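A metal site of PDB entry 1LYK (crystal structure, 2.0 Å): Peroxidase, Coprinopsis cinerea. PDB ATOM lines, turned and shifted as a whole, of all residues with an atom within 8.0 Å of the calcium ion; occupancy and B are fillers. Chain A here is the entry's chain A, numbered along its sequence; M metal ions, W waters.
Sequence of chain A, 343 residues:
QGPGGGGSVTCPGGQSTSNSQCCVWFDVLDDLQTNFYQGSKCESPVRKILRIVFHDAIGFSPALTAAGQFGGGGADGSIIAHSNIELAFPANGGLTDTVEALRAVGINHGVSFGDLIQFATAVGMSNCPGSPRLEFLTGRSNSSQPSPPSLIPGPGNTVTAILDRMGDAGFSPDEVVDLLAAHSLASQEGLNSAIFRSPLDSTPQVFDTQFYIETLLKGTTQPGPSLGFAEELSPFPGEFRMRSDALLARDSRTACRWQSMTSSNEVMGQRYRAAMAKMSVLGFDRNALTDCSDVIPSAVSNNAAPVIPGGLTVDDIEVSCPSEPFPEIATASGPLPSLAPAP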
ATOM      1  N   ILE A  52     -15.068 -24.093  21.309  1.00  0.00           N
ATOM      2  CA  ILE A  52     -16.513 -24.124  21.526  1.00  0.00           C
ATOM      3  C   ILE A  52     -17.145 -25.432  21.088  1.00  0.00           C
ATOM      4  O   ILE A  52     -17.930 -26.010  21.848  1.00  0.00           O
ATOM      5  CB  ILE A  52     -17.204 -22.935  20.782  1.00  0.00           C
ATOM      6  CG1 ILE A  52     -16.743 -21.608  21.393  1.00  0.00           C
ATOM      7  CG2 ILE A  52     -18.723 -23.103  20.797  1.00  0.00           C
ATOM      8  CD1 ILE A  52     -17.361 -20.383  20.770  1.00  0.00           C
ATOM      9  N   VAL A  53     -16.805 -25.932  19.906  1.00  0.00           N
ATOM     10  CA  VAL A  53     -17.397 -27.182  19.429  1.00  0.00           C
ATOM     11  C   VAL A  53     -17.091 -28.340  20.362  1.00  0.00           C
ATOM     12  O   VAL A  53     -17.964 -29.194  20.611  1.00  0.00           O
ATOM     13  CB  VAL A  53     -17.005 -27.514  17.970  1.00  0.00           C
ATOM     14  CG1 VAL A  53     -15.523 -27.865  17.847  1.00  0.00           C
ATOM     15  CG2 VAL A  53     -17.886 -28.628  17.436  1.00  0.00           C
ATOM     16  N   PHE A  54     -15.883 -28.355  20.917  1.00  0.00           N
ATOM     17  CA  PHE A  54     -15.503 -29.397  21.851  1.00  0.00           C
ATOM     18  C   PHE A  54     -16.259 -29.195  23.173  1.00  0.00           C
ATOM     19  O   PHE A  54     -16.843 -30.134  23.702  1.00  0.00           O
ATOM     20  CB  PHE A  54     -13.981 -29.379  22.086  1.00  0.00           C
ATOM     21  CG  PHE A  54     -13.520 -30.295  23.195  1.00  0.00           C
ATOM     22  CD1 PHE A  54     -12.616 -29.843  24.168  1.00  0.00           C
ATOM     23  CD2 PHE A  54     -14.007 -31.580  23.300  1.00  0.00           C
ATOM     24  CE1 PHE A  54     -12.203 -30.666  25.214  1.00  0.00           C
ATOM     25  CE2 PHE A  54     -13.604 -32.423  24.328  1.00  0.00           C
ATOM     26  CZ  PHE A  54     -12.699 -31.961  25.301  1.00  0.00           C
ATOM     27  N   HIS A  55     -16.277 -27.962  23.682  1.00  0.00           N
ATOM     28  CA  HIS A  55     -16.953 -27.694  24.956  1.00  0.00           C
ATOM     29  C   HIS A  55     -18.461 -27.843  24.855  1.00  0.00           C
ATOM     30  O   HIS A  55     -19.116 -28.137  25.847  1.00  0.00           O
ATOM     31  CB  HIS A  55     -16.556 -26.324  25.499  1.00  0.00           C
ATOM     32  CG  HIS A  55     -15.112 -26.232  25.908  1.00  0.00           C
ATOM     33  ND1 HIS A  55     -14.609 -25.197  26.658  1.00  0.00           N
ATOM     34  CD2 HIS A  55     -14.067 -27.070  25.675  1.00  0.00           C
ATOM     35  CE1 HIS A  55     -13.322 -25.387  26.869  1.00  0.00           C
ATOM     36  NE2 HIS A  55     -12.967 -26.518  26.287  1.00  0.00           N
ATOM     37  N   ASP A  56     -19.018 -27.643  23.674  1.00  0.00           N
ATOM     38  CA  ASP A  56     -20.454 -27.795  23.516  1.00  0.00           C
ATOM     39  C   ASP A  56     -20.861 -29.265  23.509  1.00  0.00           C
ATOM     40  O   ASP A  56     -21.853 -29.632  24.164  1.00  0.00           O
ATOM     41  CB  ASP A  56     -20.970 -27.177  22.214  1.00  0.00           C
ATOM     42  CG  ASP A  56     -22.448 -27.447  22.006  1.00  0.00           C
ATOM     43  OD1 ASP A  56     -23.222 -27.285  22.980  1.00  0.00           O
ATOM     44  OD2 ASP A  56     -22.859 -27.836  20.894  1.00  0.00           O
ATOM     45  N   ALA A  57     -20.168 -30.065  22.715  1.00  0.00           N
ATOM     46  CA  ALA A  57     -20.473 -31.490  22.570  1.00  0.00           C
ATOM     47  C   ALA A  57     -20.178 -32.407  23.750  1.00  0.00           C
ATOM     48  O   ALA A  57     -21.002 -33.273  24.097  1.00  0.00           O
ATOM     49  CB  ALA A  57     -19.816 -32.027  21.310  1.00  0.00           C
ATOM     50  N   ILE A  58     -19.048 -32.208  24.416  1.00  0.00           N
ATOM     51  CA  ILE A  58     -18.655 -33.060  25.537  1.00  0.00           C
ATOM     52  C   ILE A  58     -19.572 -32.949  26.769  1.00  0.00           C
ATOM     53  O   ILE A  58     -19.390 -33.660  27.764  1.00  0.00           O
ATOM     54  CB  ILE A  58     -17.128 -32.852  25.853  1.00  0.00           C
ATOM     55  CG1 ILE A  58     -16.534 -34.116  26.476  1.00  0.00           C
ATOM     56  CG2 ILE A  58     -16.890 -31.653  26.726  1.00  0.00           C
ATOM     57  CD1 ILE A  58     -16.409 -35.265  25.494  1.00  0.00           C
ATOM     58  N   GLY A  59     -20.563 -32.065  26.698  1.00  0.00           N
ATOM     59  CA  GLY A  59     -21.513 -31.932  27.791  1.00  0.00           C
ATOM     60  C   GLY A  59     -22.551 -33.008  27.569  1.00  0.00           C
ATOM     61  O   GLY A  59     -23.706 -32.715  27.207  1.00  0.00           O
ATOM     62  N   PHE A  60     -22.132 -34.252  27.721  1.00  0.00           N
ATOM     63  CA  PHE A  60     -22.985 -35.398  27.496  1.00  0.00           C
ATOM     64  C   PHE A  60     -22.417 -36.440  28.427  1.00  0.00           C
ATOM     65  O   PHE A  60     -21.215 -36.655  28.445  1.00  0.00           O
ATOM     66  CB  PHE A  60     -22.836 -35.847  26.031  1.00  0.00           C
ATOM     67  CG  PHE A  60     -23.630 -37.066  25.663  1.00  0.00           C
ATOM     68  CD1 PHE A  60     -25.014 -37.001  25.541  1.00  0.00           C
ATOM     69  CD2 PHE A  60     -22.995 -38.282  25.454  1.00  0.00           C
ATOM     70  CE1 PHE A  60     -25.753 -38.123  25.205  1.00  0.00           C
ATOM     71  CE2 PHE A  60     -23.722 -39.415  25.123  1.00  0.00           C
ATOM     72  CZ  PHE A  60     -25.101 -39.340  24.987  1.00  0.00           C
ATOM     73  N   GLY A  72     -26.834 -34.076  30.095  1.00  0.00           N
ATOM     74  CA  GLY A  72     -26.438 -33.107  29.091  1.00  0.00           C
ATOM     75  C   GLY A  72     -26.865 -33.585  27.706  1.00  0.00           C
ATOM     76  O   GLY A  72     -26.897 -34.785  27.456  1.00  0.00           O
ATOM     77  N   GLY A  73     -27.193 -32.646  26.822  1.00  0.00           N
ATOM     78  CA  GLY A  73     -27.633 -33.033  25.490  1.00  0.00           C
ATOM     79  C   GLY A  73     -26.596 -33.060  24.380  1.00  0.00           C
ATOM     80  O   GLY A  73     -26.961 -33.031  23.201  1.00  0.00           O
ATOM     81  N   GLY A  74     -25.313 -33.059  24.744  1.00  0.00           N
ATOM     82  CA  GLY A  74     -24.269 -33.106  23.741  1.00  0.00           C
ATOM     83  C   GLY A  74     -24.151 -31.881  22.869  1.00  0.00           C
ATOM     84  O   GLY A  74     -24.223 -30.746  23.368  1.00  0.00           O
ATOM     85  N   ALA A  75     -23.992 -32.111  21.560  1.00  0.00           N
ATOM     86  CA  ALA A  75     -23.829 -31.058  20.550  1.00  0.00           C
ATOM     87  C   ALA A  75     -25.125 -30.317  20.190  1.00  0.00           C
ATOM     88  O   ALA A  75     -25.410 -30.042  19.034  1.00  0.00           O
ATOM     89  CB  ALA A  75     -23.193 -31.654  19.276  1.00  0.00           C
ATOM     90  N   ASP A  76     -25.866 -29.956  21.231  1.00  0.00           N
ATOM     91  CA  ASP A  76     -27.140 -29.276  21.104  1.00  0.00           C
ATOM     92  C   ASP A  76     -27.106 -27.756  21.005  1.00  0.00           C
ATOM     93  O   ASP A  76     -28.155 -27.118  20.978  1.00  0.00           O
ATOM     94  CB  ASP A  76     -28.050 -29.697  22.273  1.00  0.00           C
ATOM     95  CG  ASP A  76     -27.416 -29.461  23.651  1.00  0.00           C
ATOM     96  OD1 ASP A  76     -28.001 -29.859  24.662  1.00  0.00           O
ATOM     97  OD2 ASP A  76     -26.327 -28.859  23.735  1.00  0.00           O
ATOM     98  N   GLY A  77     -25.910 -27.180  20.924  1.00  0.00           N
ATOM     99  CA  GLY A  77     -25.804 -25.734  20.843  1.00  0.00           C
ATOM    100  C   GLY A  77     -26.131 -25.054  22.168  1.00  0.00           C
ATOM    101  O   GLY A  77     -26.334 -23.841  22.210  1.00  0.00           O
ATOM    102  N   SER A  78     -26.110 -25.836  23.251  1.00  0.00           N
ATOM    103  CA  SER A  78     -26.420 -25.328  24.586  1.00  0.00           C
ATOM    104  C   SER A  78     -25.462 -24.268  25.102  1.00  0.00           C
ATOM    105  O   SER A  78     -25.831 -23.447  25.939  1.00  0.00           O
ATOM    106  CB  SER A  78     -26.512 -26.464  25.615  1.00  0.00           C
ATOM    107  OG  SER A  78     -25.288 -27.172  25.754  1.00  0.00           O
ATOM    108  N   ILE A  79     -24.224 -24.316  24.629  1.00  0.00           N
ATOM    109  CA  ILE A  79     -23.225 -23.338  25.056  1.00  0.00           C
ATOM    110  C   ILE A  79     -23.642 -21.934  24.595  1.00  0.00           C
ATOM    111  O   ILE A  79     -23.284 -20.931  25.215  1.00  0.00           O
ATOM    112  CB  ILE A  79     -21.809 -23.736  24.530  1.00  0.00           C
ATOM    113  CG1 ILE A  79     -20.726 -22.903  25.213  1.00  0.00           C
ATOM    114  CG2 ILE A  79     -21.729 -23.620  23.002  1.00  0.00           C
ATOM    115  CD1 ILE A  79     -19.351 -23.498  25.059  1.00  0.00           C
ATOM    116  N   ILE A  80     -24.414 -21.862  23.516  1.00  0.00           N
ATOM    117  CA  ILE A  80     -24.887 -20.575  23.046  1.00  0.00           C
ATOM    118  C   ILE A  80     -26.239 -20.301  23.693  1.00  0.00           C
ATOM    119  O   ILE A  80     -26.395 -19.291  24.375  1.00  0.00           O
ATOM    120  CB  ILE A  80     -25.029 -20.518  21.502  1.00  0.00           C
ATOM    121  CG1 ILE A  80     -23.673 -20.722  20.833  1.00  0.00           C
ATOM    122  CG2 ILE A  80     -25.560 -19.137  21.086  1.00  0.00           C
ATOM    123  CD1 ILE A  80     -23.740 -20.598  19.321  1.00  0.00           C
ATOM    124  N   HIS A  82     -27.644 -21.385  26.358  1.00  0.00           N
ATOM    125  CA  HIS A  82     -27.540 -21.170  27.794  1.00  0.00           C
ATOM    126  C   HIS A  82     -26.180 -20.643  28.188  1.00  0.00           C
ATOM    127  O   HIS A  82     -25.644 -21.022  29.230  1.00  0.00           O
ATOM    128  CB  HIS A  82     -27.845 -22.465  28.544  1.00  0.00           C
ATOM    129  CG  HIS A  82     -29.172 -23.044  28.199  1.00  0.00           C
ATOM    130  ND1 HIS A  82     -30.353 -22.529  28.690  1.00  0.00           N
ATOM    131  CD2 HIS A  82     -29.520 -24.037  27.351  1.00  0.00           C
ATOM    132  CE1 HIS A  82     -31.369 -23.165  28.146  1.00  0.00           C
ATOM    133  NE2 HIS A  82     -30.893 -24.093  27.332  1.00  0.00           N
ATOM    134  N   GLU A  86     -23.439 -21.792  31.126  1.00  0.00           N
ATOM    135  CA  GLU A  86     -22.235 -22.458  30.653  1.00  0.00           C
ATOM    136  C   GLU A  86     -20.975 -21.615  30.582  1.00  0.00           C
ATOM    137  O   GLU A  86     -19.902 -22.094  30.912  1.00  0.00           O
ATOM    138  CB  GLU A  86     -22.500 -23.145  29.328  1.00  0.00           C
ATOM    139  CG  GLU A  86     -23.567 -24.229  29.432  1.00  0.00           C
ATOM    140  CD  GLU A  86     -23.633 -25.117  28.216  1.00  0.00           C
ATOM    141  OE1 GLU A  86     -22.642 -25.201  27.472  1.00  0.00           O
ATOM    142  OE2 GLU A  86     -24.687 -25.751  28.025  1.00  0.00           O
ATOM    143  N   GLY A 114     -26.916 -25.825  17.476  1.00  0.00           N
ATOM    144  CA  GLY A 114     -26.190 -27.076  17.389  1.00  0.00           C
ATOM    145  C   GLY A 114     -25.575 -27.250  16.003  1.00  0.00           C
ATOM    146  O   GLY A 114     -24.379 -27.515  15.878  1.00  0.00           O
ATOM    147  N   ILE A 117     -22.744 -24.390  15.137  1.00  0.00           N
ATOM    148  CA  ILE A 117     -21.423 -24.641  15.697  1.00  0.00           C
ATOM    149  C   ILE A 117     -20.669 -25.654  14.845  1.00  0.00           C
ATOM    150  O   ILE A 117     -19.509 -25.437  14.527  1.00  0.00           O
ATOM    151  CB  ILE A 117     -21.518 -25.106  17.168  1.00  0.00           C
ATOM    152  CG1 ILE A 117     -21.904 -23.923  18.067  1.00  0.00           C
ATOM    153  CG2 ILE A 117     -20.216 -25.738  17.639  1.00  0.00           C
ATOM    154  CD1 ILE A 117     -22.412 -24.336  19.441  1.00  0.00           C
ATOM    155  N   SER A 144     -32.748 -26.888  23.957  1.00  0.00           N
ATOM    156  CA  SER A 144     -31.750 -27.542  24.788  1.00  0.00           C
ATOM    157  C   SER A 144     -31.855 -27.106  26.254  1.00  0.00           C
ATOM    158  O   SER A 144     -32.474 -26.090  26.561  1.00  0.00           O
ATOM    159  CB  SER A 144     -30.354 -27.218  24.257  1.00  0.00           C
ATOM    160  OG  SER A 144     -30.077 -25.821  24.281  1.00  0.00           O
ATOM    161  N   GLN A 145     -31.264 -27.908  27.135  1.00  0.00           N
ATOM    162  CA  GLN A 145     -31.193 -27.631  28.567  1.00  0.00           C
ATOM    163  C   GLN A 145     -29.718 -27.321  28.811  1.00  0.00           C
ATOM    164  O   GLN A 145     -28.851 -27.789  28.062  1.00  0.00           O
ATOM    165  CB  GLN A 145     -31.584 -28.862  29.383  1.00  0.00           C
ATOM    166  CG  GLN A 145     -33.079 -29.161  29.461  1.00  0.00           C
ATOM    167  CD  GLN A 145     -33.401 -30.335  30.413  1.00  0.00           C
ATOM    168  OE1 GLN A 145     -33.581 -31.477  29.992  1.00  0.00           O
ATOM    169  NE2 GLN A 145     -33.476 -30.040  31.704  1.00  0.00           N
ATOM    170  N   PRO A 146     -29.392 -26.457  29.787  1.00  0.00           N
ATOM    171  CA  PRO A 146     -27.965 -26.204  29.986  1.00  0.00           C
ATOM    172  C   PRO A 146     -27.194 -27.447  30.422  1.00  0.00           C
ATOM    173  O   PRO A 146     -27.726 -28.339  31.094  1.00  0.00           O
ATOM    174  CB  PRO A 146     -27.950 -25.112  31.054  1.00  0.00           C
ATOM    175  CG  PRO A 146     -29.209 -25.354  31.809  1.00  0.00           C
ATOM    176  CD  PRO A 146     -30.197 -25.641  30.715  1.00  0.00           C
ATOM    177  N   SER A 147     -25.954 -27.534  29.980  1.00  0.00           N
ATOM    178  CA  SER A 147     -25.100 -28.662  30.323  1.00  0.00           C
ATOM    179  C   SER A 147     -24.751 -28.630  31.802  1.00  0.00           C
ATOM    180  O   SER A 147     -24.707 -27.551  32.409  1.00  0.00           O
ATOM    181  CB  SER A 147     -23.799 -28.563  29.533  1.00  0.00           C
ATOM    182  OG  SER A 147     -22.866 -29.565  29.907  1.00  0.00           O
ATOM    183  N   PRO A 148     -24.615 -29.819  32.416  1.00  0.00           N
ATOM    184  CA  PRO A 148     -24.244 -29.879  33.837  1.00  0.00           C
ATOM    185  C   PRO A 148     -22.789 -29.387  33.884  1.00  0.00           C
ATOM    186  O   PRO A 148     -22.099 -29.375  32.856  1.00  0.00           O
ATOM    187  CB  PRO A 148     -24.292 -31.379  34.133  1.00  0.00           C
ATOM    188  CG  PRO A 148     -25.389 -31.850  33.221  1.00  0.00           C
ATOM    189  CD  PRO A 148     -25.085 -31.126  31.944  1.00  0.00           C
ATOM    190  N   LEU A 282     -23.002 -36.392  19.259  1.00  0.00           N
ATOM    191  CA  LEU A 282     -23.237 -36.739  20.657  1.00  0.00           C
ATOM    192  C   LEU A 282     -24.568 -36.106  21.058  1.00  0.00           C
ATOM    193  O   LEU A 282     -24.757 -34.904  20.903  1.00  0.00           O
ATOM    194  CB  LEU A 282     -22.136 -36.207  21.569  1.00  0.00           C
ATOM    195  CG  LEU A 282     -20.755 -36.843  21.477  1.00  0.00           C
ATOM    196  CD1 LEU A 282     -19.830 -36.172  22.467  1.00  0.00           C
ATOM    197  CD2 LEU A 282     -20.859 -38.320  21.768  1.00  0.00           C
ATOM    198  N   PHE A 284     -27.380 -37.195  19.722  1.00  0.00           N
ATOM    199  CA  PHE A 284     -28.286 -37.377  18.602  1.00  0.00           C
ATOM    200  C   PHE A 284     -28.157 -38.736  17.902  1.00  0.00           C
ATOM    201  O   PHE A 284     -27.322 -39.563  18.262  1.00  0.00           O
ATOM    202  CB  PHE A 284     -28.104 -36.246  17.574  1.00  0.00           C
ATOM    203  CG  PHE A 284     -28.290 -34.873  18.157  1.00  0.00           C
ATOM    204  CD1 PHE A 284     -29.542 -34.265  18.129  1.00  0.00           C
ATOM    205  CD2 PHE A 284     -27.218 -34.190  18.719  1.00  0.00           C
ATOM    206  CE1 PHE A 284     -29.720 -33.003  18.672  1.00  0.00           C
ATOM    207  CE2 PHE A 284     -27.391 -32.929  19.271  1.00  0.00           C
ATOM    208  CZ  PHE A 284     -28.644 -32.340  19.243  1.00  0.00           C
HETATM  209 CA    CA M   1     -24.016 -28.873  24.764  1.00  0.00          CA
HETATM  210  O   HOH W   1     -22.607 -27.848  26.428  1.00  0.00           O
HETATM  211  O   HOH W   2     -24.476 -30.240  26.546  1.00  0.00           O
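The calcium ion is bound by water W2 (2.3 Å), the backbone carbonyl oxygen of Gly 74 (2.3 Å), the side-chain hydroxyl of Ser 78 (2.3 Å), the backbone carbonyl oxygen of Asp 56 (2.4 Å), water W1 (2.4 Å), the side-chain carboxylate of Asp 56 (2.5 Å) and the side-chain carboxylate of Asp 76 (2.5 Å). The calcium ion has seven donor atoms within binding distance.
The side-chain hydroxyl (OG) of Ser 78 lies close to the side-chain carboxylate (OE2) of Glu 86 (2.7 Å). The backbone NH of Gly 74 lies within hydrogen-bond range of the backbone carbonyl oxygen of Gly 59, at 3.0 Å. The backbone NH (N) of Gly 77 lies within hydrogen-bond range of the side-chain carboxylate (OD2) of Asp 56.
Water W2 lies within hydrogen-bond range of O of Gly 59 and N of Gly 74.
Within 4 Å of the calcium ion: Asp 56, Gly 74, Asp 76 and Ser 78.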
